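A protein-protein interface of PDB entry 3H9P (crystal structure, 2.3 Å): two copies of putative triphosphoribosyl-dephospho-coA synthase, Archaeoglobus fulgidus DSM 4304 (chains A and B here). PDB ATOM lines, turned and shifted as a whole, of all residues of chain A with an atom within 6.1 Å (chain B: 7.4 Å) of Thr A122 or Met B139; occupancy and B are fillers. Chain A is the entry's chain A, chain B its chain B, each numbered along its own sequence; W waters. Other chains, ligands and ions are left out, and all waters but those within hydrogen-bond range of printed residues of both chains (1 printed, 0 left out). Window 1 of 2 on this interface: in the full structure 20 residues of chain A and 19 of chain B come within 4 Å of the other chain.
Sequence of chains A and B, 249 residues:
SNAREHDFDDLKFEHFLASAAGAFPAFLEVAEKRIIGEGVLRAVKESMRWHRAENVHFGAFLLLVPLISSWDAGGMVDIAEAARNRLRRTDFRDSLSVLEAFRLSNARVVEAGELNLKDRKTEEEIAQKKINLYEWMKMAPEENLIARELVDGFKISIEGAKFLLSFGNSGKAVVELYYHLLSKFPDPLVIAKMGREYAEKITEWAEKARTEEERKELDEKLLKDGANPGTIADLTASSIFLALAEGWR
Of the 16 printed residues of chain A, 6 touch a printed residue of chain B.
Hydrophobic or aromatic side chains of chain A within 4 Å of the printed part of chain B: Ile A131.
Printed residues of chain B that touch a printed residue of chain A: Ile B131, Glu B135, Lys B138, Met B139, Glu B142 and Val B151.
Hydrophobic or aromatic side chains of chain B within 4 Å of the printed part of chain A: Ile B131, Met B139 and Val B151.
Among the printed residues, 11 pairs touch across the chains.
Among the printed residues, Asp or Glu carboxylates within 4 Å of a Lys or Arg side-chain nitrogen of the other chain: Glu A124 with Lys B138 and Glu A125 with Lys B138.
Water W1 lies within hydrogen-bond range of the side-chain hydroxyl of Thr A122 (2.8 Å) and the backbone carbonyl oxygen of Ala B140 (3.3 Å).
Among the printed residues, merely in contact across the chains: Lys A118 with Glu B142, Lys A121 with Lys B138, Lys A121 with Val B151, Thr A122 with Met B139, Glu A125 with Glu B135, Glu A125 with Met B139, Ile A131 with Ile B131 and Ile A131 with Met B139.
Ile B131 touches its own counterpart, Ile A131.
Ile A131 touches Met B139, but with the chains exchanged Met A139 does not touch Ile B131 (4.1 Å).
Of the 11 pairs that touch across the chains among the printed residues, 1 has its exchanged pair printed and touching as well.
The side-chain amino group (NZ) of Lys B138 is in salt-bridge range of the side-chain carboxylate (OE2) of Glu A125, 3.0 Å away.
The side-chain carboxylate (OE1) of Glu A124 is in salt-bridge range of the side-chain amino group (NZ) of Lys B138.
N of Thr A122 lies within hydrogen-bond range of O of Lys B138 (3.4 Å).
Arg A120 touches none of the printed residues of chain B.
Thr A122 touches two residues of chain B.
Printed residues of chain B within 4 Å of Ile A131: Ile B131 (3.9 Å) and Met B139 (3.7 Å).
Of the printed residues of chain A, Glu B135 touches Glu A125.
The nearest residue of chain A that does not touch Met B139 is Met A139 (4.3 Å).
The nearest printed residue of chain A that does not touch Glu B142 is Asp A119 (6.2 Å).
The backbone carbonyl oxygen of Ile B126 lies within hydrogen-bond range of the backbone NH of Ile B131, 2.9 Å away.
OD1 of Asn B132 lies within hydrogen-bond range of N of Glu B135.
The backbone NH (N) of Ile A131 lies within hydrogen-bond range of the backbone carbonyl oxygen (O) of Ile A126, at 3.0 Å.
The side-chain hydroxyl of Thr A122 lies within hydrogen-bond range of the backbone carbonyl oxygen of Lys A118 (2.9 Å).
The backbone carbonyl oxygen (O) of Val B151 lies within hydrogen-bond range of the side-chain hydroxyl (OH) of Tyr B134, 3.4 Å away.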
ATOM      1  N   LEU A  96     -26.317  35.094  13.329  1.00  0.00           N
ATOM      2  CA  LEU A  96     -27.555  34.350  13.516  1.00  0.00           C
ATOM      3  C   LEU A  96     -28.789  35.239  13.248  1.00  0.00           C
ATOM      4  O   LEU A  96     -29.714  34.829  12.548  1.00  0.00           O
ATOM      5  CB  LEU A  96     -27.600  33.741  14.947  1.00  0.00           C
ATOM      6  CG  LEU A  96     -26.650  32.571  15.244  1.00  0.00           C
ATOM      7  CD1 LEU A  96     -26.726  32.057  16.710  1.00  0.00           C
ATOM      8  CD2 LEU A  96     -26.906  31.402  14.290  1.00  0.00           C
ATOM      9  N   LEU A  99     -28.862  35.857   9.530  1.00  0.00           N
ATOM     10  CA  LEU A  99     -29.383  34.651   8.902  1.00  0.00           C
ATOM     11  C   LEU A  99     -30.910  34.491   9.046  1.00  0.00           C
ATOM     12  O   LEU A  99     -31.615  34.227   8.066  1.00  0.00           O
ATOM     13  CB  LEU A  99     -28.634  33.419   9.436  1.00  0.00           C
ATOM     14  CG  LEU A  99     -28.892  32.063   8.774  1.00  0.00           C
ATOM     15  CD1 LEU A  99     -28.830  32.156   7.238  1.00  0.00           C
ATOM     16  CD2 LEU A  99     -27.871  31.050   9.264  1.00  0.00           C
ATOM     17  N   LEU A 117     -33.239  22.195   7.724  1.00  0.00           N
ATOM     18  CA  LEU A 117     -32.066  21.867   8.540  1.00  0.00           C
ATOM     19  C   LEU A 117     -30.734  22.173   7.814  1.00  0.00           C
ATOM     20  O   LEU A 117     -29.655  21.761   8.249  1.00  0.00           O
ATOM     21  CB  LEU A 117     -32.130  20.394   9.023  1.00  0.00           C
ATOM     22  N   LYS A 118     -30.819  22.882   6.690  1.00  0.00           N
ATOM     23  CA  LYS A 118     -29.616  23.449   6.072  1.00  0.00           C
ATOM     24  C   LYS A 118     -29.303  24.715   6.886  1.00  0.00           C
ATOM     25  O   LYS A 118     -28.193  24.849   7.435  1.00  0.00           O
ATOM     26  CB  LYS A 118     -29.841  23.761   4.554  1.00  0.00           C
ATOM     27  N   ASP A 119     -30.313  25.596   7.007  1.00  0.00           N
ATOM     28  CA  ASP A 119     -30.270  26.738   7.929  1.00  0.00           C
ATOM     29  C   ASP A 119     -29.890  26.291   9.347  1.00  0.00           C
ATOM     30  O   ASP A 119     -29.081  26.946  10.017  1.00  0.00           O
ATOM     31  CB  ASP A 119     -31.602  27.480   7.940  1.00  0.00           C
ATOM     32  N   ARG A 120     -30.464  25.168   9.773  1.00  0.00           N
ATOM     33  CA  ARG A 120     -30.195  24.579  11.084  1.00  0.00           C
ATOM     34  C   ARG A 120     -28.729  24.188  11.269  1.00  0.00           C
ATOM     35  O   ARG A 120     -28.143  24.445  12.316  1.00  0.00           O
ATOM     36  CB  ARG A 120     -31.076  23.356  11.275  1.00  0.00           C
ATOM     37  CG  ARG A 120     -31.000  22.717  12.653  1.00  0.00           C
ATOM     38  CD  ARG A 120     -32.288  21.970  12.940  1.00  0.00           C
ATOM     39  NE  ARG A 120     -33.433  22.761  12.495  1.00  0.00           N
ATOM     40  CZ  ARG A 120     -34.656  22.284  12.288  1.00  0.00           C
ATOM     41  NH1 ARG A 120     -34.931  20.994  12.494  1.00  0.00           N
ATOM     42  NH2 ARG A 120     -35.612  23.113  11.876  1.00  0.00           N
ATOM     43  N   LYS A 121     -28.159  23.552  10.251  1.00  0.00           N
ATOM     44  CA  LYS A 121     -26.765  23.140  10.273  1.00  0.00           C
ATOM     45  C   LYS A 121     -25.794  24.314  10.148  1.00  0.00           C
ATOM     46  O   LYS A 121     -24.747  24.342  10.788  1.00  0.00           O
ATOM     47  CB  LYS A 121     -26.521  22.068   9.208  1.00  0.00           C
ATOM     48  CG  LYS A 121     -27.065  20.705   9.690  1.00  0.00           C
ATOM     49  CD  LYS A 121     -27.207  19.700   8.593  1.00  0.00           C
ATOM     50  CE  LYS A 121     -27.847  18.437   9.141  1.00  0.00           C
ATOM     51  NZ  LYS A 121     -27.786  17.353   8.145  1.00  0.00           N
ATOM     52  N   THR A 122     -26.176  25.292   9.346  1.00  0.00           N
ATOM     53  CA  THR A 122     -25.405  26.503   9.246  1.00  0.00           C
ATOM     54  C   THR A 122     -25.415  27.250  10.573  1.00  0.00           C
ATOM     55  O   THR A 122     -24.344  27.621  11.084  1.00  0.00           O
ATOM     56  CB  THR A 122     -25.882  27.397   8.106  1.00  0.00           C
ATOM     57  OG1 THR A 122     -25.943  26.619   6.902  1.00  0.00           O
ATOM     58  CG2 THR A 122     -24.895  28.529   7.896  1.00  0.00           C
ATOM     59  N   GLU A 123     -26.614  27.430  11.135  1.00  0.00           N
ATOM     60  CA  GLU A 123     -26.767  28.119  12.407  1.00  0.00           C
ATOM     61  C   GLU A 123     -25.930  27.430  13.462  1.00  0.00           C
ATOM     62  O   GLU A 123     -25.253  28.082  14.255  1.00  0.00           O
ATOM     63  CB  GLU A 123     -28.222  28.121  12.873  1.00  0.00           C
ATOM     64  CG  GLU A 123     -29.155  29.003  12.076  1.00  0.00           C
ATOM     65  CD  GLU A 123     -30.609  28.585  12.229  1.00  0.00           C
ATOM     66  OE1 GLU A 123     -30.878  27.498  12.787  1.00  0.00           O
ATOM     67  OE2 GLU A 123     -31.493  29.336  11.781  1.00  0.00           O
ATOM     68  N   GLU A 124     -25.953  26.104  13.463  1.00  0.00           N
ATOM     69  CA  GLU A 124     -25.246  25.405  14.520  1.00  0.00           C
ATOM     70  C   GLU A 124     -23.726  25.513  14.377  1.00  0.00           C
ATOM     71  O   GLU A 124     -23.034  25.562  15.376  1.00  0.00           O
ATOM     72  CB  GLU A 124     -25.776  23.979  14.753  1.00  0.00           C
ATOM     73  CG  GLU A 124     -25.313  22.887  13.812  1.00  0.00           C
ATOM     74  CD  GLU A 124     -25.983  21.541  14.128  1.00  0.00           C
ATOM     75  OE1 GLU A 124     -25.262  20.577  14.493  1.00  0.00           O
ATOM     76  OE2 GLU A 124     -27.237  21.449  14.039  1.00  0.00           O
ATOM     77  N   GLU A 125     -23.214  25.625  13.151  1.00  0.00           N
ATOM     78  CA  GLU A 125     -21.770  25.821  12.972  1.00  0.00           C
ATOM     79  C   GLU A 125     -21.322  27.250  13.204  1.00  0.00           C
ATOM     80  O   GLU A 125     -20.241  27.481  13.759  1.00  0.00           O
ATOM     81  CB  GLU A 125     -21.283  25.299  11.626  1.00  0.00           C
ATOM     82  CG  GLU A 125     -21.399  23.824  11.543  1.00  0.00           C
ATOM     83  CD  GLU A 125     -20.671  23.106  12.676  1.00  0.00           C
ATOM     84  OE1 GLU A 125     -19.461  23.362  12.858  1.00  0.00           O
ATOM     85  OE2 GLU A 125     -21.322  22.291  13.383  1.00  0.00           O
ATOM     86  N   ILE A 126     -22.158  28.200  12.802  1.00  0.00           N
ATOM     87  CA  ILE A 126     -21.960  29.579  13.222  1.00  0.00           C
ATOM     88  C   ILE A 126     -21.797  29.667  14.733  1.00  0.00           C
ATOM     89  O   ILE A 126     -20.776  30.147  15.222  1.00  0.00           O
ATOM     90  CB  ILE A 126     -23.066  30.535  12.741  1.00  0.00           C
ATOM     91  CG1 ILE A 126     -22.997  30.671  11.214  1.00  0.00           C
ATOM     92  CG2 ILE A 126     -22.855  31.912  13.363  1.00  0.00           C
ATOM     93  CD1 ILE A 126     -24.269  31.177  10.601  1.00  0.00           C
ATOM     94  N   ALA A 127     -22.786  29.159  15.459  1.00  0.00           N
ATOM     95  CA  ALA A 127     -22.702  29.076  16.919  1.00  0.00           C
ATOM     96  C   ALA A 127     -21.401  28.410  17.399  1.00  0.00           C
ATOM     97  O   ALA A 127     -20.591  29.046  18.073  1.00  0.00           O
ATOM     98  CB  ALA A 127     -23.928  28.354  17.483  1.00  0.00           C
ATOM     99  N   ILE A 131     -18.649  32.273  14.724  1.00  0.00           N
ATOM    100  CA  ILE A 131     -18.342  32.984  13.500  1.00  0.00           C
ATOM    101  C   ILE A 131     -19.137  34.268  13.456  1.00  0.00           C
ATOM    102  O   ILE A 131     -20.373  34.268  13.256  1.00  0.00           O
ATOM    103  CB  ILE A 131     -18.549  32.129  12.227  1.00  0.00           C
ATOM    104  CG1 ILE A 131     -17.759  30.815  12.359  1.00  0.00           C
ATOM    105  CG2 ILE A 131     -18.133  32.922  11.005  1.00  0.00           C
ATOM    106  CD1 ILE A 131     -17.745  29.884  11.100  1.00  0.00           C
ATOM    107  N   TRP A 136     -17.981  35.487   8.770  1.00  0.00           N
ATOM    108  CA  TRP A 136     -18.922  34.823   7.896  1.00  0.00           C
ATOM    109  C   TRP A 136     -18.796  35.402   6.490  1.00  0.00           C
ATOM    110  O   TRP A 136     -18.545  34.666   5.532  1.00  0.00           O
ATOM    111  CB  TRP A 136     -20.339  35.010   8.426  1.00  0.00           C
ATOM    112  CG  TRP A 136     -21.323  34.058   7.823  1.00  0.00           C
ATOM    113  CD1 TRP A 136     -21.047  32.875   7.209  1.00  0.00           C
ATOM    114  CD2 TRP A 136     -22.749  34.179   7.837  1.00  0.00           C
ATOM    115  NE1 TRP A 136     -22.206  32.265   6.804  1.00  0.00           N
ATOM    116  CE2 TRP A 136     -23.270  33.033   7.186  1.00  0.00           C
ATOM    117  CE3 TRP A 136     -23.643  35.155   8.327  1.00  0.00           C
ATOM    118  CZ2 TRP A 136     -24.653  32.824   7.003  1.00  0.00           C
ATOM    119  CZ3 TRP A 136     -25.036  34.954   8.137  1.00  0.00           C
ATOM    120  CH2 TRP A 136     -25.518  33.795   7.478  1.00  0.00           C
ATOM    121  N   MET A 139     -16.186  34.478   4.142  1.00  0.00           N
ATOM    122  CA  MET A 139     -16.250  33.157   3.504  1.00  0.00           C
ATOM    123  C   MET A 139     -17.225  33.068   2.323  1.00  0.00           C
ATOM    124  O   MET A 139     -17.428  32.006   1.757  1.00  0.00           O
ATOM    125  CB  MET A 139     -16.571  32.095   4.532  1.00  0.00           C
ATOM    126  CG  MET A 139     -15.446  31.911   5.485  1.00  0.00           C
ATOM    127  SD  MET A 139     -15.970  30.797   6.974  1.00  0.00           S
ATOM    128  CE  MET A 139     -17.751  31.448   7.340  1.00  0.00           C
ATOM    129  N   ILE B 126     -10.628  29.404   7.667  1.00  0.00           N
ATOM    130  CA  ILE B 126     -10.636  27.957   7.905  1.00  0.00           C
ATOM    131  C   ILE B 126      -9.542  27.602   8.886  1.00  0.00           C
ATOM    132  O   ILE B 126      -9.754  26.849   9.849  1.00  0.00           O
ATOM    133  CB  ILE B 126     -10.470  27.177   6.582  1.00  0.00           C
ATOM    134  CG1 ILE B 126     -11.830  27.080   5.880  1.00  0.00           C
ATOM    135  CG2 ILE B 126      -9.835  25.800   6.820  1.00  0.00           C
ATOM    136  CD1 ILE B 126     -11.710  26.929   4.405  1.00  0.00           C
ATOM    137  N   ILE B 131     -11.766  25.102  10.920  1.00  0.00           N
ATOM    138  CA  ILE B 131     -12.980  24.530  10.385  1.00  0.00           C
ATOM    139  C   ILE B 131     -12.620  23.241   9.628  1.00  0.00           C
ATOM    140  O   ILE B 131     -11.980  23.280   8.557  1.00  0.00           O
ATOM    141  CB  ILE B 131     -13.726  25.539   9.490  1.00  0.00           C
ATOM    142  CG1 ILE B 131     -14.220  26.709  10.345  1.00  0.00           C
ATOM    143  CG2 ILE B 131     -14.907  24.895   8.777  1.00  0.00           C
ATOM    144  CD1 ILE B 131     -14.778  27.882   9.549  1.00  0.00           C
ATOM    145  N   ASN B 132     -13.058  22.107  10.169  1.00  0.00           N
ATOM    146  CA  ASN B 132     -12.811  20.865   9.494  1.00  0.00           C
ATOM    147  C   ASN B 132     -13.756  20.659   8.342  1.00  0.00           C
ATOM    148  O   ASN B 132     -14.618  21.497   8.062  1.00  0.00           O
ATOM    149  CB  ASN B 132     -12.777  19.666  10.460  1.00  0.00           C
ATOM    150  CG  ASN B 132     -14.150  19.101  10.793  1.00  0.00           C
ATOM    151  OD1 ASN B 132     -15.161  19.330  10.108  1.00  0.00           O
ATOM    152  ND2 ASN B 132     -14.167  18.278  11.827  1.00  0.00           N
ATOM    153  N   LEU B 133     -13.585  19.539   7.675  1.00  0.00           N
ATOM    154  CA  LEU B 133     -14.223  19.349   6.390  1.00  0.00           C
ATOM    155  C   LEU B 133     -15.719  19.202   6.559  1.00  0.00           C
ATOM    156  O   LEU B 133     -16.505  19.717   5.778  1.00  0.00           O
ATOM    157  CB  LEU B 133     -13.641  18.118   5.691  1.00  0.00           C
ATOM    158  CG  LEU B 133     -14.123  17.873   4.265  1.00  0.00           C
ATOM    159  CD1 LEU B 133     -13.992  19.196   3.455  1.00  0.00           C
ATOM    160  CD2 LEU B 133     -13.303  16.729   3.622  1.00  0.00           C
ATOM    161  N   TYR B 134     -16.092  18.477   7.606  1.00  0.00           N
ATOM    162  CA  TYR B 134     -17.469  18.234   7.962  1.00  0.00           C
ATOM    163  C   TYR B 134     -18.141  19.537   8.370  1.00  0.00           C
ATOM    164  O   TYR B 134     -19.227  19.844   7.900  1.00  0.00           O
ATOM    165  CB  TYR B 134     -17.477  17.232   9.119  1.00  0.00           C
ATOM    166  CG  TYR B 134     -18.823  16.822   9.586  1.00  0.00           C
ATOM    167  CD1 TYR B 134     -19.494  15.750   8.950  1.00  0.00           C
ATOM    168  CD2 TYR B 134     -19.427  17.445  10.678  1.00  0.00           C
ATOM    169  CE1 TYR B 134     -20.731  15.334   9.370  1.00  0.00           C
ATOM    170  CE2 TYR B 134     -20.705  17.018  11.131  1.00  0.00           C
ATOM    171  CZ  TYR B 134     -21.327  15.967  10.449  1.00  0.00           C
ATOM    172  OH  TYR B 134     -22.540  15.496  10.818  1.00  0.00           O
ATOM    173  N   GLU B 135     -17.489  20.319   9.230  1.00  0.00           N
ATOM    174  CA  GLU B 135     -18.078  21.580   9.711  1.00  0.00           C
ATOM    175  C   GLU B 135     -18.273  22.578   8.549  1.00  0.00           C
ATOM    176  O   GLU B 135     -19.223  23.359   8.529  1.00  0.00           O
ATOM    177  CB  GLU B 135     -17.177  22.201  10.781  1.00  0.00           C
ATOM    178  CG  GLU B 135     -17.048  21.373  12.083  1.00  0.00           C
ATOM    179  CD  GLU B 135     -15.781  21.678  12.907  1.00  0.00           C
ATOM    180  OE1 GLU B 135     -14.729  22.054  12.357  1.00  0.00           O
ATOM    181  OE2 GLU B 135     -15.817  21.502  14.140  1.00  0.00           O
ATOM    182  N   TRP B 136     -17.319  22.567   7.620  1.00  0.00           N
ATOM    183  CA  TRP B 136     -17.317  23.433   6.454  1.00  0.00           C
ATOM    184  C   TRP B 136     -18.459  23.054   5.540  1.00  0.00           C
ATOM    185  O   TRP B 136     -19.188  23.916   5.110  1.00  0.00           O
ATOM    186  CB  TRP B 136     -16.006  23.305   5.689  1.00  0.00           C
ATOM    187  CG  TRP B 136     -15.837  24.315   4.615  1.00  0.00           C
ATOM    188  CD1 TRP B 136     -16.378  25.563   4.580  1.00  0.00           C
ATOM    189  CD2 TRP B 136     -15.005  24.205   3.459  1.00  0.00           C
ATOM    190  NE1 TRP B 136     -15.965  26.226   3.456  1.00  0.00           N
ATOM    191  CE2 TRP B 136     -15.120  25.415   2.747  1.00  0.00           C
ATOM    192  CE3 TRP B 136     -14.169  23.197   2.947  1.00  0.00           C
ATOM    193  CZ2 TRP B 136     -14.441  25.646   1.531  1.00  0.00           C
ATOM    194  CZ3 TRP B 136     -13.493  23.426   1.726  1.00  0.00           C
ATOM    195  CH2 TRP B 136     -13.642  24.639   1.039  1.00  0.00           C
ATOM    196  N   MET B 137     -18.617  21.755   5.273  1.00  0.00           N
ATOM    197  CA  MET B 137     -19.742  21.278   4.497  1.00  0.00           C
ATOM    198  C   MET B 137     -21.074  21.592   5.195  1.00  0.00           C
ATOM    199  O   MET B 137     -22.071  21.819   4.542  1.00  0.00           O
ATOM    200  CB  MET B 137     -19.609  19.765   4.226  1.00  0.00           C
ATOM    201  CG  MET B 137     -18.459  19.371   3.296  1.00  0.00           C
ATOM    202  SD  MET B 137     -18.492  20.351   1.561  1.00  0.00           S
ATOM    203  CE  MET B 137     -17.023  21.621   1.947  1.00  0.00           C
ATOM    204  N   LYS B 138     -21.085  21.621   6.525  1.00  0.00           N
ATOM    205  CA  LYS B 138     -22.323  21.972   7.239  1.00  0.00           C
ATOM    206  C   LYS B 138     -22.822  23.403   7.000  1.00  0.00           C
ATOM    207  O   LYS B 138     -23.972  23.711   7.282  1.00  0.00           O
ATOM    208  CB  LYS B 138     -22.165  21.731   8.741  1.00  0.00           C
ATOM    209  CG  LYS B 138     -22.220  20.275   9.096  1.00  0.00           C
ATOM    210  CD  LYS B 138     -22.348  20.098  10.599  1.00  0.00           C
ATOM    211  CE  LYS B 138     -23.673  20.651  11.103  1.00  0.00           C
ATOM    212  NZ  LYS B 138     -23.618  20.619  12.560  1.00  0.00           N
ATOM    213  N   MET B 139     -21.955  24.260   6.463  1.00  0.00           N
ATOM    214  CA  MET B 139     -22.298  25.661   6.243  1.00  0.00           C
ATOM    215  C   MET B 139     -22.591  25.957   4.783  1.00  0.00           C
ATOM    216  O   MET B 139     -22.718  27.115   4.398  1.00  0.00           O
ATOM    217  CB  MET B 139     -21.146  26.558   6.688  1.00  0.00           C
ATOM    218  CG  MET B 139     -20.909  26.535   8.167  1.00  0.00           C
ATOM    219  SD  MET B 139     -19.395  27.674   8.592  1.00  0.00           S
ATOM    220  CE  MET B 139     -17.974  26.840   7.561  1.00  0.00           C
ATOM    221  N   ALA B 140     -22.654  24.905   3.977  1.00  0.00           N
ATOM    222  CA  ALA B 140     -22.883  25.044   2.546  1.00  0.00           C
ATOM    223  C   ALA B 140     -24.359  25.358   2.262  1.00  0.00           C
ATOM    224  O   ALA B 140     -25.226  25.090   3.092  1.00  0.00           O
ATOM    225  CB  ALA B 140     -22.459  23.781   1.837  1.00  0.00           C
ATOM    226  N   PRO B 141     -24.653  25.946   1.091  1.00  0.00           N
ATOM    227  CA  PRO B 141     -26.067  26.181   0.719  1.00  0.00           C
ATOM    228  C   PRO B 141     -26.873  24.889   0.671  1.00  0.00           C
ATOM    229  O   PRO B 141     -26.339  23.850   0.291  1.00  0.00           O
ATOM    230  CB  PRO B 141     -25.968  26.773  -0.687  1.00  0.00           C
ATOM    231  CG  PRO B 141     -24.609  27.383  -0.746  1.00  0.00           C
ATOM    232  CD  PRO B 141     -23.711  26.573   0.150  1.00  0.00           C
ATOM    233  N   GLU B 142     -28.134  24.960   1.089  1.00  0.00           N
ATOM    234  CA  GLU B 142     -29.171  23.924   0.865  1.00  0.00           C
ATOM    235  C   GLU B 142     -28.970  23.110  -0.433  1.00  0.00           C
ATOM    236  O   GLU B 142     -28.919  21.873  -0.407  1.00  0.00           O
ATOM    237  CB  GLU B 142     -30.582  24.595   0.874  1.00  0.00           C
ATOM    238  CG  GLU B 142     -31.797  23.653   0.616  1.00  0.00           C
ATOM    239  CD  GLU B 142     -33.175  24.386   0.471  1.00  0.00           C
ATOM    240  OE1 GLU B 142     -33.332  25.548   0.929  1.00  0.00           O
ATOM    241  OE2 GLU B 142     -34.126  23.781  -0.093  1.00  0.00           O
ATOM    242  N   ALA B 147     -22.229  18.534  -0.525  1.00  0.00           N
ATOM    243  CA  ALA B 147     -22.078  18.976   0.873  1.00  0.00           C
ATOM    244  C   ALA B 147     -23.042  18.227   1.797  1.00  0.00           C
ATOM    245  O   ALA B 147     -22.636  17.690   2.827  1.00  0.00           O
ATOM    246  CB  ALA B 147     -22.282  20.516   1.016  1.00  0.00           C
ATOM    247  N   VAL B 151     -22.408  15.407   4.891  1.00  0.00           N
ATOM    248  CA  VAL B 151     -22.849  15.718   6.220  1.00  0.00           C
ATOM    249  C   VAL B 151     -23.896  14.709   6.737  1.00  0.00           C
ATOM    250  O   VAL B 151     -23.940  14.402   7.929  1.00  0.00           O
ATOM    251  CB  VAL B 151     -23.436  17.164   6.250  1.00  0.00           C
ATOM    252  CG1 VAL B 151     -24.367  17.316   7.391  1.00  0.00           C
ATOM    253  CG2 VAL B 151     -22.310  18.187   6.322  1.00  0.00           C
HETATM  254  O   HOH W   1     -26.557  27.845   4.406  1.00  0.00           O
